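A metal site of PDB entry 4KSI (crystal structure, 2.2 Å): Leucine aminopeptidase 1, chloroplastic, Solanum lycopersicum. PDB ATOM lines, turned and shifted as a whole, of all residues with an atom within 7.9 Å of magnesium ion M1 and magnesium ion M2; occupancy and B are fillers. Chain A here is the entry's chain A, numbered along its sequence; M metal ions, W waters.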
ATOM      1  N   VAL A 268      30.700 -10.172 -15.595  1.00  0.00           N
ATOM      2  CA  VAL A 268      30.251 -11.531 -15.224  1.00  0.00           C
ATOM      3  C   VAL A 268      30.270 -11.652 -13.690  1.00  0.00           C
ATOM      4  O   VAL A 268      29.305 -12.164 -13.065  1.00  0.00           O
ATOM      5  CB  VAL A 268      31.165 -12.636 -15.821  1.00  0.00           C
ATOM      6  CG1 VAL A 268      30.754 -13.998 -15.263  1.00  0.00           C
ATOM      7  CG2 VAL A 268      31.133 -12.592 -17.368  1.00  0.00           C
ATOM      8  N   LYS A 300      39.348 -21.397 -18.176  1.00  0.00           N
ATOM      9  CA  LYS A 300      38.119 -20.794 -17.770  1.00  0.00           C
ATOM     10  C   LYS A 300      37.901 -21.173 -16.310  1.00  0.00           C
ATOM     11  O   LYS A 300      37.945 -22.361 -15.954  1.00  0.00           O
ATOM     12  CB  LYS A 300      36.967 -21.353 -18.611  1.00  0.00           C
ATOM     13  CG  LYS A 300      35.603 -20.845 -18.135  1.00  0.00           C
ATOM     14  CD  LYS A 300      34.455 -21.503 -18.918  1.00  0.00           C
ATOM     15  CE  LYS A 300      33.133 -21.206 -18.244  1.00  0.00           C
ATOM     16  NZ  LYS A 300      32.025 -21.860 -18.996  1.00  0.00           N
ATOM     17  N   GLY A 301      37.676 -20.172 -15.467  1.00  0.00           N
ATOM     18  CA  GLY A 301      37.624 -20.431 -14.045  1.00  0.00           C
ATOM     19  C   GLY A 301      36.325 -19.959 -13.397  1.00  0.00           C
ATOM     20  O   GLY A 301      36.327 -19.203 -12.417  1.00  0.00           O
ATOM     21  N   LEU A 302      35.218 -20.474 -13.915  1.00  0.00           N
ATOM     22  CA  LEU A 302      33.910 -20.222 -13.300  1.00  0.00           C
ATOM     23  C   LEU A 302      33.747 -21.265 -12.186  1.00  0.00           C
ATOM     24  O   LEU A 302      33.362 -22.442 -12.449  1.00  0.00           O
ATOM     25  CB  LEU A 302      32.775 -20.318 -14.367  1.00  0.00           C
ATOM     26  CG  LEU A 302      32.419 -18.990 -15.084  1.00  0.00           C
ATOM     27  CD1 LEU A 302      31.656 -18.036 -14.145  1.00  0.00           C
ATOM     28  CD2 LEU A 302      33.702 -18.259 -15.516  1.00  0.00           C
ATOM     29  N   PHE A 304      31.461 -21.483 -10.084  1.00  0.00           N
ATOM     30  CA  PHE A 304      30.079 -21.940 -10.264  1.00  0.00           C
ATOM     31  C   PHE A 304      29.424 -21.119 -11.359  1.00  0.00           C
ATOM     32  O   PHE A 304      29.689 -19.922 -11.503  1.00  0.00           O
ATOM     33  CB  PHE A 304      29.203 -21.848  -8.999  1.00  0.00           C
ATOM     34  CG  PHE A 304      27.878 -22.538  -9.182  1.00  0.00           C
ATOM     35  CD1 PHE A 304      27.808 -23.943  -9.246  1.00  0.00           C
ATOM     36  CD2 PHE A 304      26.718 -21.800  -9.446  1.00  0.00           C
ATOM     37  CE1 PHE A 304      26.589 -24.598  -9.533  1.00  0.00           C
ATOM     38  CE2 PHE A 304      25.511 -22.424  -9.676  1.00  0.00           C
ATOM     39  CZ  PHE A 304      25.451 -23.834  -9.727  1.00  0.00           C
ATOM     40  N   ASP A 305      28.495 -21.733 -12.100  1.00  0.00           N
ATOM     41  CA  ASP A 305      27.785 -21.008 -13.146  1.00  0.00           C
ATOM     42  C   ASP A 305      26.308 -21.319 -13.034  1.00  0.00           C
ATOM     43  O   ASP A 305      25.854 -22.421 -13.412  1.00  0.00           O
ATOM     44  CB  ASP A 305      28.288 -21.420 -14.534  1.00  0.00           C
ATOM     45  CG  ASP A 305      27.557 -20.697 -15.671  1.00  0.00           C
ATOM     46  OD1 ASP A 305      26.890 -19.652 -15.438  1.00  0.00           O
ATOM     47  OD2 ASP A 305      27.639 -21.193 -16.839  1.00  0.00           O
ATOM     48  N   SER A 306      25.533 -20.362 -12.499  1.00  0.00           N
ATOM     49  CA  SER A 306      24.086 -20.538 -12.455  1.00  0.00           C
ATOM     50  C   SER A 306      23.480 -20.224 -13.841  1.00  0.00           C
ATOM     51  O   SER A 306      22.356 -20.525 -14.061  1.00  0.00           O
ATOM     52  CB  SER A 306      23.437 -19.605 -11.406  1.00  0.00           C
ATOM     53  OG  SER A 306      23.616 -18.223 -11.799  1.00  0.00           O
ATOM     54  N   GLY A 307      24.223 -19.554 -14.737  1.00  0.00           N
ATOM     55  CA  GLY A 307      23.593 -18.963 -15.939  1.00  0.00           C
ATOM     56  C   GLY A 307      23.352 -17.468 -15.767  1.00  0.00           C
ATOM     57  O   GLY A 307      23.202 -16.741 -16.762  1.00  0.00           O
ATOM     58  N   GLY A 308      23.331 -16.962 -14.513  1.00  0.00           N
ATOM     59  CA  GLY A 308      23.020 -15.535 -14.262  1.00  0.00           C
ATOM     60  C   GLY A 308      21.538 -15.350 -14.574  1.00  0.00           C
ATOM     61  O   GLY A 308      20.741 -16.317 -14.457  1.00  0.00           O
ATOM     62  N   ASN A 310      20.008 -15.345 -17.287  1.00  0.00           N
ATOM     63  CA  ASN A 310      19.651 -16.443 -18.172  1.00  0.00           C
ATOM     64  C   ASN A 310      19.884 -17.749 -17.393  1.00  0.00           C
ATOM     65  O   ASN A 310      20.708 -18.611 -17.778  1.00  0.00           O
ATOM     66  CB  ASN A 310      20.512 -16.367 -19.444  1.00  0.00           C
ATOM     67  CG  ASN A 310      19.977 -15.324 -20.460  1.00  0.00           C
ATOM     68  OD1 ASN A 310      18.940 -15.563 -21.173  1.00  0.00           O
ATOM     69  ND2 ASN A 310      20.664 -14.232 -20.560  1.00  0.00           N
ATOM     70  N   LYS A 312      20.113 -21.322 -15.823  1.00  0.00           N
ATOM     71  CA  LYS A 312      20.037 -22.711 -16.306  1.00  0.00           C
ATOM     72  C   LYS A 312      18.778 -23.418 -15.792  1.00  0.00           C
ATOM     73  O   LYS A 312      18.610 -23.621 -14.587  1.00  0.00           O
ATOM     74  CB  LYS A 312      21.291 -23.443 -15.839  1.00  0.00           C
ATOM     75  CG  LYS A 312      22.560 -22.997 -16.558  1.00  0.00           C
ATOM     76  CD  LYS A 312      23.796 -23.677 -15.976  1.00  0.00           C
ATOM     77  CE  LYS A 312      25.101 -23.148 -16.613  1.00  0.00           C
ATOM     78  NZ  LYS A 312      25.019 -23.402 -18.109  1.00  0.00           N
ATOM     79  N   MET A 322      27.600 -27.612 -12.045  1.00  0.00           N
ATOM     80  CA  MET A 322      28.353 -26.448 -12.557  1.00  0.00           C
ATOM     81  C   MET A 322      29.534 -25.996 -11.697  1.00  0.00           C
ATOM     82  O   MET A 322      30.242 -25.042 -12.060  1.00  0.00           O
ATOM     83  CB  MET A 322      27.439 -25.271 -12.949  1.00  0.00           C
ATOM     84  CG  MET A 322      26.537 -25.520 -14.179  1.00  0.00           C
ATOM     85  SD  MET A 322      27.533 -25.900 -15.666  1.00  0.00           S
ATOM     86  CE  MET A 322      27.491 -27.714 -15.764  1.00  0.00           C
ATOM     87  N   ASN A 324      31.850 -27.719 -11.999  1.00  0.00           N
ATOM     88  CA  ASN A 324      32.910 -28.179 -12.894  1.00  0.00           C
ATOM     89  C   ASN A 324      33.168 -27.188 -14.038  1.00  0.00           C
ATOM     90  O   ASN A 324      33.968 -27.474 -14.952  1.00  0.00           O
ATOM     91  CB  ASN A 324      32.618 -29.566 -13.448  1.00  0.00           C
ATOM     92  CG  ASN A 324      31.483 -29.563 -14.410  1.00  0.00           C
ATOM     93  OD1 ASN A 324      31.037 -28.501 -14.839  1.00  0.00           O
ATOM     94  ND2 ASN A 324      31.004 -30.748 -14.756  1.00  0.00           N
ATOM     95  N   ASP A 325      32.511 -26.028 -13.964  1.00  0.00           N
ATOM     96  CA  ASP A 325      32.772 -24.978 -14.952  1.00  0.00           C
ATOM     97  C   ASP A 325      34.116 -24.281 -14.743  1.00  0.00           C
ATOM     98  O   ASP A 325      34.439 -23.325 -15.459  1.00  0.00           O
ATOM     99  CB  ASP A 325      31.643 -23.971 -14.894  1.00  0.00           C
ATOM    100  CG  ASP A 325      31.159 -23.574 -16.286  1.00  0.00           C
ATOM    101  OD1 ASP A 325      31.237 -24.371 -17.280  1.00  0.00           O
ATOM    102  OD2 ASP A 325      30.671 -22.420 -16.378  1.00  0.00           O
ATOM    103  N   MET A 326      34.846 -24.704 -13.715  1.00  0.00           N
ATOM    104  CA  MET A 326      36.258 -24.286 -13.581  1.00  0.00           C
ATOM    105  C   MET A 326      37.192 -25.459 -14.023  1.00  0.00           C
ATOM    106  O   MET A 326      38.382 -25.443 -13.735  1.00  0.00           O
ATOM    107  CB  MET A 326      36.613 -23.748 -12.165  1.00  0.00           C
ATOM    108  CG  MET A 326      35.972 -24.487 -10.986  1.00  0.00           C
ATOM    109  SD  MET A 326      36.516 -26.216 -11.036  1.00  0.00           S
ATOM    110  CE  MET A 326      38.273 -26.075 -10.556  1.00  0.00           C
ATOM    111  N   ASN A 358      29.187 -17.102 -11.383  1.00  0.00           N
ATOM    112  CA  ASN A 358      28.193 -16.395 -12.195  1.00  0.00           C
ATOM    113  C   ASN A 358      26.847 -16.568 -11.451  1.00  0.00           C
ATOM    114  O   ASN A 358      26.243 -17.655 -11.501  1.00  0.00           O
ATOM    115  CB  ASN A 358      28.107 -17.031 -13.609  1.00  0.00           C
ATOM    116  CG  ASN A 358      27.188 -16.233 -14.600  1.00  0.00           C
ATOM    117  OD1 ASN A 358      26.982 -15.025 -14.428  1.00  0.00           O
ATOM    118  ND2 ASN A 358      26.684 -16.895 -15.652  1.00  0.00           N
ATOM    119  N   ASN A 383      23.027 -13.272 -23.970  1.00  0.00           N
ATOM    120  CA  ASN A 383      22.701 -14.396 -23.067  1.00  0.00           C
ATOM    121  C   ASN A 383      23.731 -14.439 -21.953  1.00  0.00           C
ATOM    122  O   ASN A 383      24.915 -14.576 -22.245  1.00  0.00           O
ATOM    123  CB  ASN A 383      22.666 -15.755 -23.832  1.00  0.00           C
ATOM    124  CG  ASN A 383      22.090 -16.912 -22.975  1.00  0.00           C
ATOM    125  OD1 ASN A 383      22.433 -17.088 -21.785  1.00  0.00           O
ATOM    126  ND2 ASN A 383      21.216 -17.742 -23.598  1.00  0.00           N
ATOM    127  N   THR A 384      23.327 -14.265 -20.714  1.00  0.00           N
ATOM    128  CA  THR A 384      24.321 -14.190 -19.640  1.00  0.00           C
ATOM    129  C   THR A 384      24.893 -15.533 -19.277  1.00  0.00           C
ATOM    130  O   THR A 384      25.794 -15.610 -18.441  1.00  0.00           O
ATOM    131  CB  THR A 384      23.746 -13.557 -18.332  1.00  0.00           C
ATOM    132  OG1 THR A 384      22.720 -14.422 -17.811  1.00  0.00           O
ATOM    133  CG2 THR A 384      23.152 -12.145 -18.622  1.00  0.00           C
ATOM    134  N   ASP A 385      24.342 -16.590 -19.859  1.00  0.00           N
ATOM    135  CA  ASP A 385      24.863 -17.921 -19.627  1.00  0.00           C
ATOM    136  C   ASP A 385      25.995 -18.266 -20.630  1.00  0.00           C
ATOM    137  O   ASP A 385      26.563 -19.374 -20.617  1.00  0.00           O
ATOM    138  CB  ASP A 385      23.744 -18.961 -19.699  1.00  0.00           C
ATOM    139  CG  ASP A 385      24.204 -20.340 -19.168  1.00  0.00           C
ATOM    140  OD1 ASP A 385      25.299 -20.480 -18.493  1.00  0.00           O
ATOM    141  OD2 ASP A 385      23.487 -21.297 -19.401  1.00  0.00           O
ATOM    142  N   ALA A 386      26.336 -17.333 -21.518  1.00  0.00           N
ATOM    143  CA  ALA A 386      27.530 -17.494 -22.308  1.00  0.00           C
ATOM    144  C   ALA A 386      28.590 -16.531 -21.719  1.00  0.00           C
ATOM    145  O   ALA A 386      29.143 -15.663 -22.414  1.00  0.00           O
ATOM    146  CB  ALA A 386      27.237 -17.229 -23.810  1.00  0.00           C
ATOM    147  N   GLU A 387      28.886 -16.720 -20.424  1.00  0.00           N
ATOM    148  CA  GLU A 387      29.667 -15.763 -19.629  1.00  0.00           C
ATOM    149  C   GLU A 387      31.133 -16.158 -19.612  1.00  0.00           C
ATOM    150  O   GLU A 387      32.012 -15.336 -19.408  1.00  0.00           O
ATOM    151  CB  GLU A 387      29.131 -15.741 -18.163  1.00  0.00           C
ATOM    152  CG  GLU A 387      29.597 -16.934 -17.280  1.00  0.00           C
ATOM    153  CD  GLU A 387      29.140 -18.308 -17.783  1.00  0.00           C
ATOM    154  OE1 GLU A 387      27.966 -18.503 -18.234  1.00  0.00           O
ATOM    155  OE2 GLU A 387      29.978 -19.248 -17.756  1.00  0.00           O
ATOM    156  N   GLY A 388      31.406 -17.437 -19.868  1.00  0.00           N
ATOM    157  CA  GLY A 388      32.794 -17.907 -19.822  1.00  0.00           C
ATOM    158  C   GLY A 388      33.627 -17.236 -20.883  1.00  0.00           C
ATOM    159  O   GLY A 388      34.798 -16.828 -20.626  1.00  0.00           O
ATOM    160  N   ARG A 389      33.050 -17.059 -22.072  1.00  0.00           N
ATOM    161  CA  ARG A 389      33.811 -16.393 -23.127  1.00  0.00           C
ATOM    162  C   ARG A 389      34.112 -14.903 -22.795  1.00  0.00           C
ATOM    163  O   ARG A 389      35.081 -14.360 -23.314  1.00  0.00           O
ATOM    164  CB  ARG A 389      33.087 -16.527 -24.475  1.00  0.00           C
ATOM    165  CG  ARG A 389      31.729 -15.784 -24.492  1.00  0.00           C
ATOM    166  CD  ARG A 389      30.866 -16.319 -25.681  1.00  0.00           C
ATOM    167  NE  ARG A 389      30.504 -17.720 -25.482  1.00  0.00           N
ATOM    168  CZ  ARG A 389      29.901 -18.486 -26.403  1.00  0.00           C
ATOM    169  NH1 ARG A 389      29.542 -17.970 -27.609  1.00  0.00           N
ATOM    170  NH2 ARG A 389      29.600 -19.726 -26.105  1.00  0.00           N
ATOM    171  N   THR A 391      34.762 -13.766 -19.616  1.00  0.00           N
ATOM    172  CA  THR A 391      35.921 -13.796 -18.720  1.00  0.00           C
ATOM    173  C   THR A 391      37.186 -14.150 -19.515  1.00  0.00           C
ATOM    174  O   THR A 391      38.241 -13.581 -19.269  1.00  0.00           O
ATOM    175  CB  THR A 391      35.738 -14.765 -17.555  1.00  0.00           C
ATOM    176  OG1 THR A 391      35.818 -16.092 -18.047  1.00  0.00           O
ATOM    177  CG2 THR A 391      34.373 -14.569 -16.926  1.00  0.00           C
ATOM    178  N   THR A 412      35.366 -25.197 -20.391  1.00  0.00           N
ATOM    179  CA  THR A 412      34.058 -25.874 -20.476  1.00  0.00           C
ATOM    180  C   THR A 412      33.042 -24.954 -21.167  1.00  0.00           C
ATOM    181  O   THR A 412      32.229 -24.346 -20.497  1.00  0.00           O
ATOM    182  CB  THR A 412      33.532 -26.210 -19.078  1.00  0.00           C
ATOM    183  OG1 THR A 412      33.709 -25.073 -18.233  1.00  0.00           O
ATOM    184  CG2 THR A 412      34.397 -27.383 -18.462  1.00  0.00           C
ATOM    185  N   LEU A 413      33.135 -24.762 -22.464  1.00  0.00           N
ATOM    186  CA  LEU A 413      32.474 -23.610 -23.029  1.00  0.00           C
ATOM    187  C   LEU A 413      31.044 -23.897 -23.455  1.00  0.00           C
ATOM    188  O   LEU A 413      30.159 -23.098 -23.184  1.00  0.00           O
ATOM    189  CB  LEU A 413      33.251 -23.031 -24.227  1.00  0.00           C
ATOM    190  CG  LEU A 413      33.088 -21.491 -24.390  1.00  0.00           C
ATOM    191  CD1 LEU A 413      33.963 -20.718 -23.382  1.00  0.00           C
ATOM    192  CD2 LEU A 413      33.431 -21.028 -25.814  1.00  0.00           C
ATOM    193  N   THR A 414      30.791 -25.009 -24.136  1.00  0.00           N
ATOM    194  CA  THR A 414      29.479 -25.128 -24.810  1.00  0.00           C
ATOM    195  C   THR A 414      28.895 -26.525 -24.617  1.00  0.00           C
ATOM    196  O   THR A 414      29.670 -27.527 -24.598  1.00  0.00           O
ATOM    197  CB  THR A 414      29.520 -24.795 -26.338  1.00  0.00           C
ATOM    198  OG1 THR A 414      30.303 -25.793 -27.022  1.00  0.00           O
ATOM    199  CG2 THR A 414      30.135 -23.413 -26.597  1.00  0.00           C
HETATM  200 MG    MG M   1      27.356 -20.362 -18.688  1.00  0.00          MG
HETATM  201 MG    MG M   2      30.062 -21.344 -17.920  1.00  0.00          MG
HETATM  202  O   HOH W   1      28.661 -23.573 -18.357  1.00  0.00           O
HETATM  203  O   HOH W   2      28.315 -21.546 -19.680  1.00  0.00           O
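The backbone carbonyl oxygen (O) of Asp 325 is in hydrogen-bond range of the backbone NH (N) of Leu 302.
The side-chain carboxylate (OD1) of Asp 325 is in hydrogen-bond range of the side-chain hydroxyl (OG1) of Thr 412 (2.7 Å).
The side-chain amino group (NZ) of Lys 312 sits close to the side-chain carboxylate (OD2) of Asp 305.
The side-chain carboxylate (OD1) of Asp 305 is in hydrogen-bond range of the backbone NH (N) of Gly 307 (2.8 Å).
The side-chain amino group (NZ) of Lys 312 lies within salt-bridge range of the side-chain carboxylate (OD2) of Asp 385.
The backbone carbonyl oxygen of Gly 307 is in hydrogen-bond range of the backbone NH of Asp 385, 3.3 Å away.
The side-chain amino group (NZ) of Lys 300 lies close to the backbone carbonyl oxygen (O) of Thr 412, at 2.9 Å.
N of Lys 312 is in hydrogen-bond range of O of Ser 306, at 3.0 Å.
Lys 312 touches magnesium ion M1 (NZ to MG, 3.9 Å).
Four residues have an atom within 4 Å of magnesium ion M1: Asp 305, Lys 312, Asp 385 and Glu 387.
The nearest printed residue that does not touch magnesium ion M1 is Ala 386 (4.3 Å).
Within 4 Å of magnesium ion M2: Lys 300, Asp 305, Asp 325 and Glu 387.
The nearest printed residue that does not touch magnesium ion M2 is Leu 302 (4.4 Å).
Magnesium ion M1 is bound by water W2 (1.8 Å), the side-chain carboxylate of Glu 387 (2.0 Å), the side-chain carboxylate of Asp 305 (2.0 Å), the side-chain carboxylate of Asp 385 (2.1 Å) and the backbone carbonyl oxygen of Asp 385 (2.3 Å).
Magnesium ion M1 has five donor atoms within binding distance.
Magnesium ion M2 is bound by the side-chain carboxylate (OD2) of Asp 325 (2.0 Å), the side-chain carboxylate (OE2) of Glu 387 (2.1 Å), the side-chain amino group (NZ) of Lys 300 (2.3 Å) and water W2 (2.5 Å).
Magnesium ion M2 has four donor atoms within binding distance.
Slightly farther from magnesium ion M2 lies OD2 of Asp 305 (2.7 Å).
Slightly farther from magnesium ion M2 lies water W1 (2.7 Å).
Water W1 lies within hydrogen-bond range of OD1 of Asp 325 (2.9 Å) and SD of Met 322 (3.7 Å).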
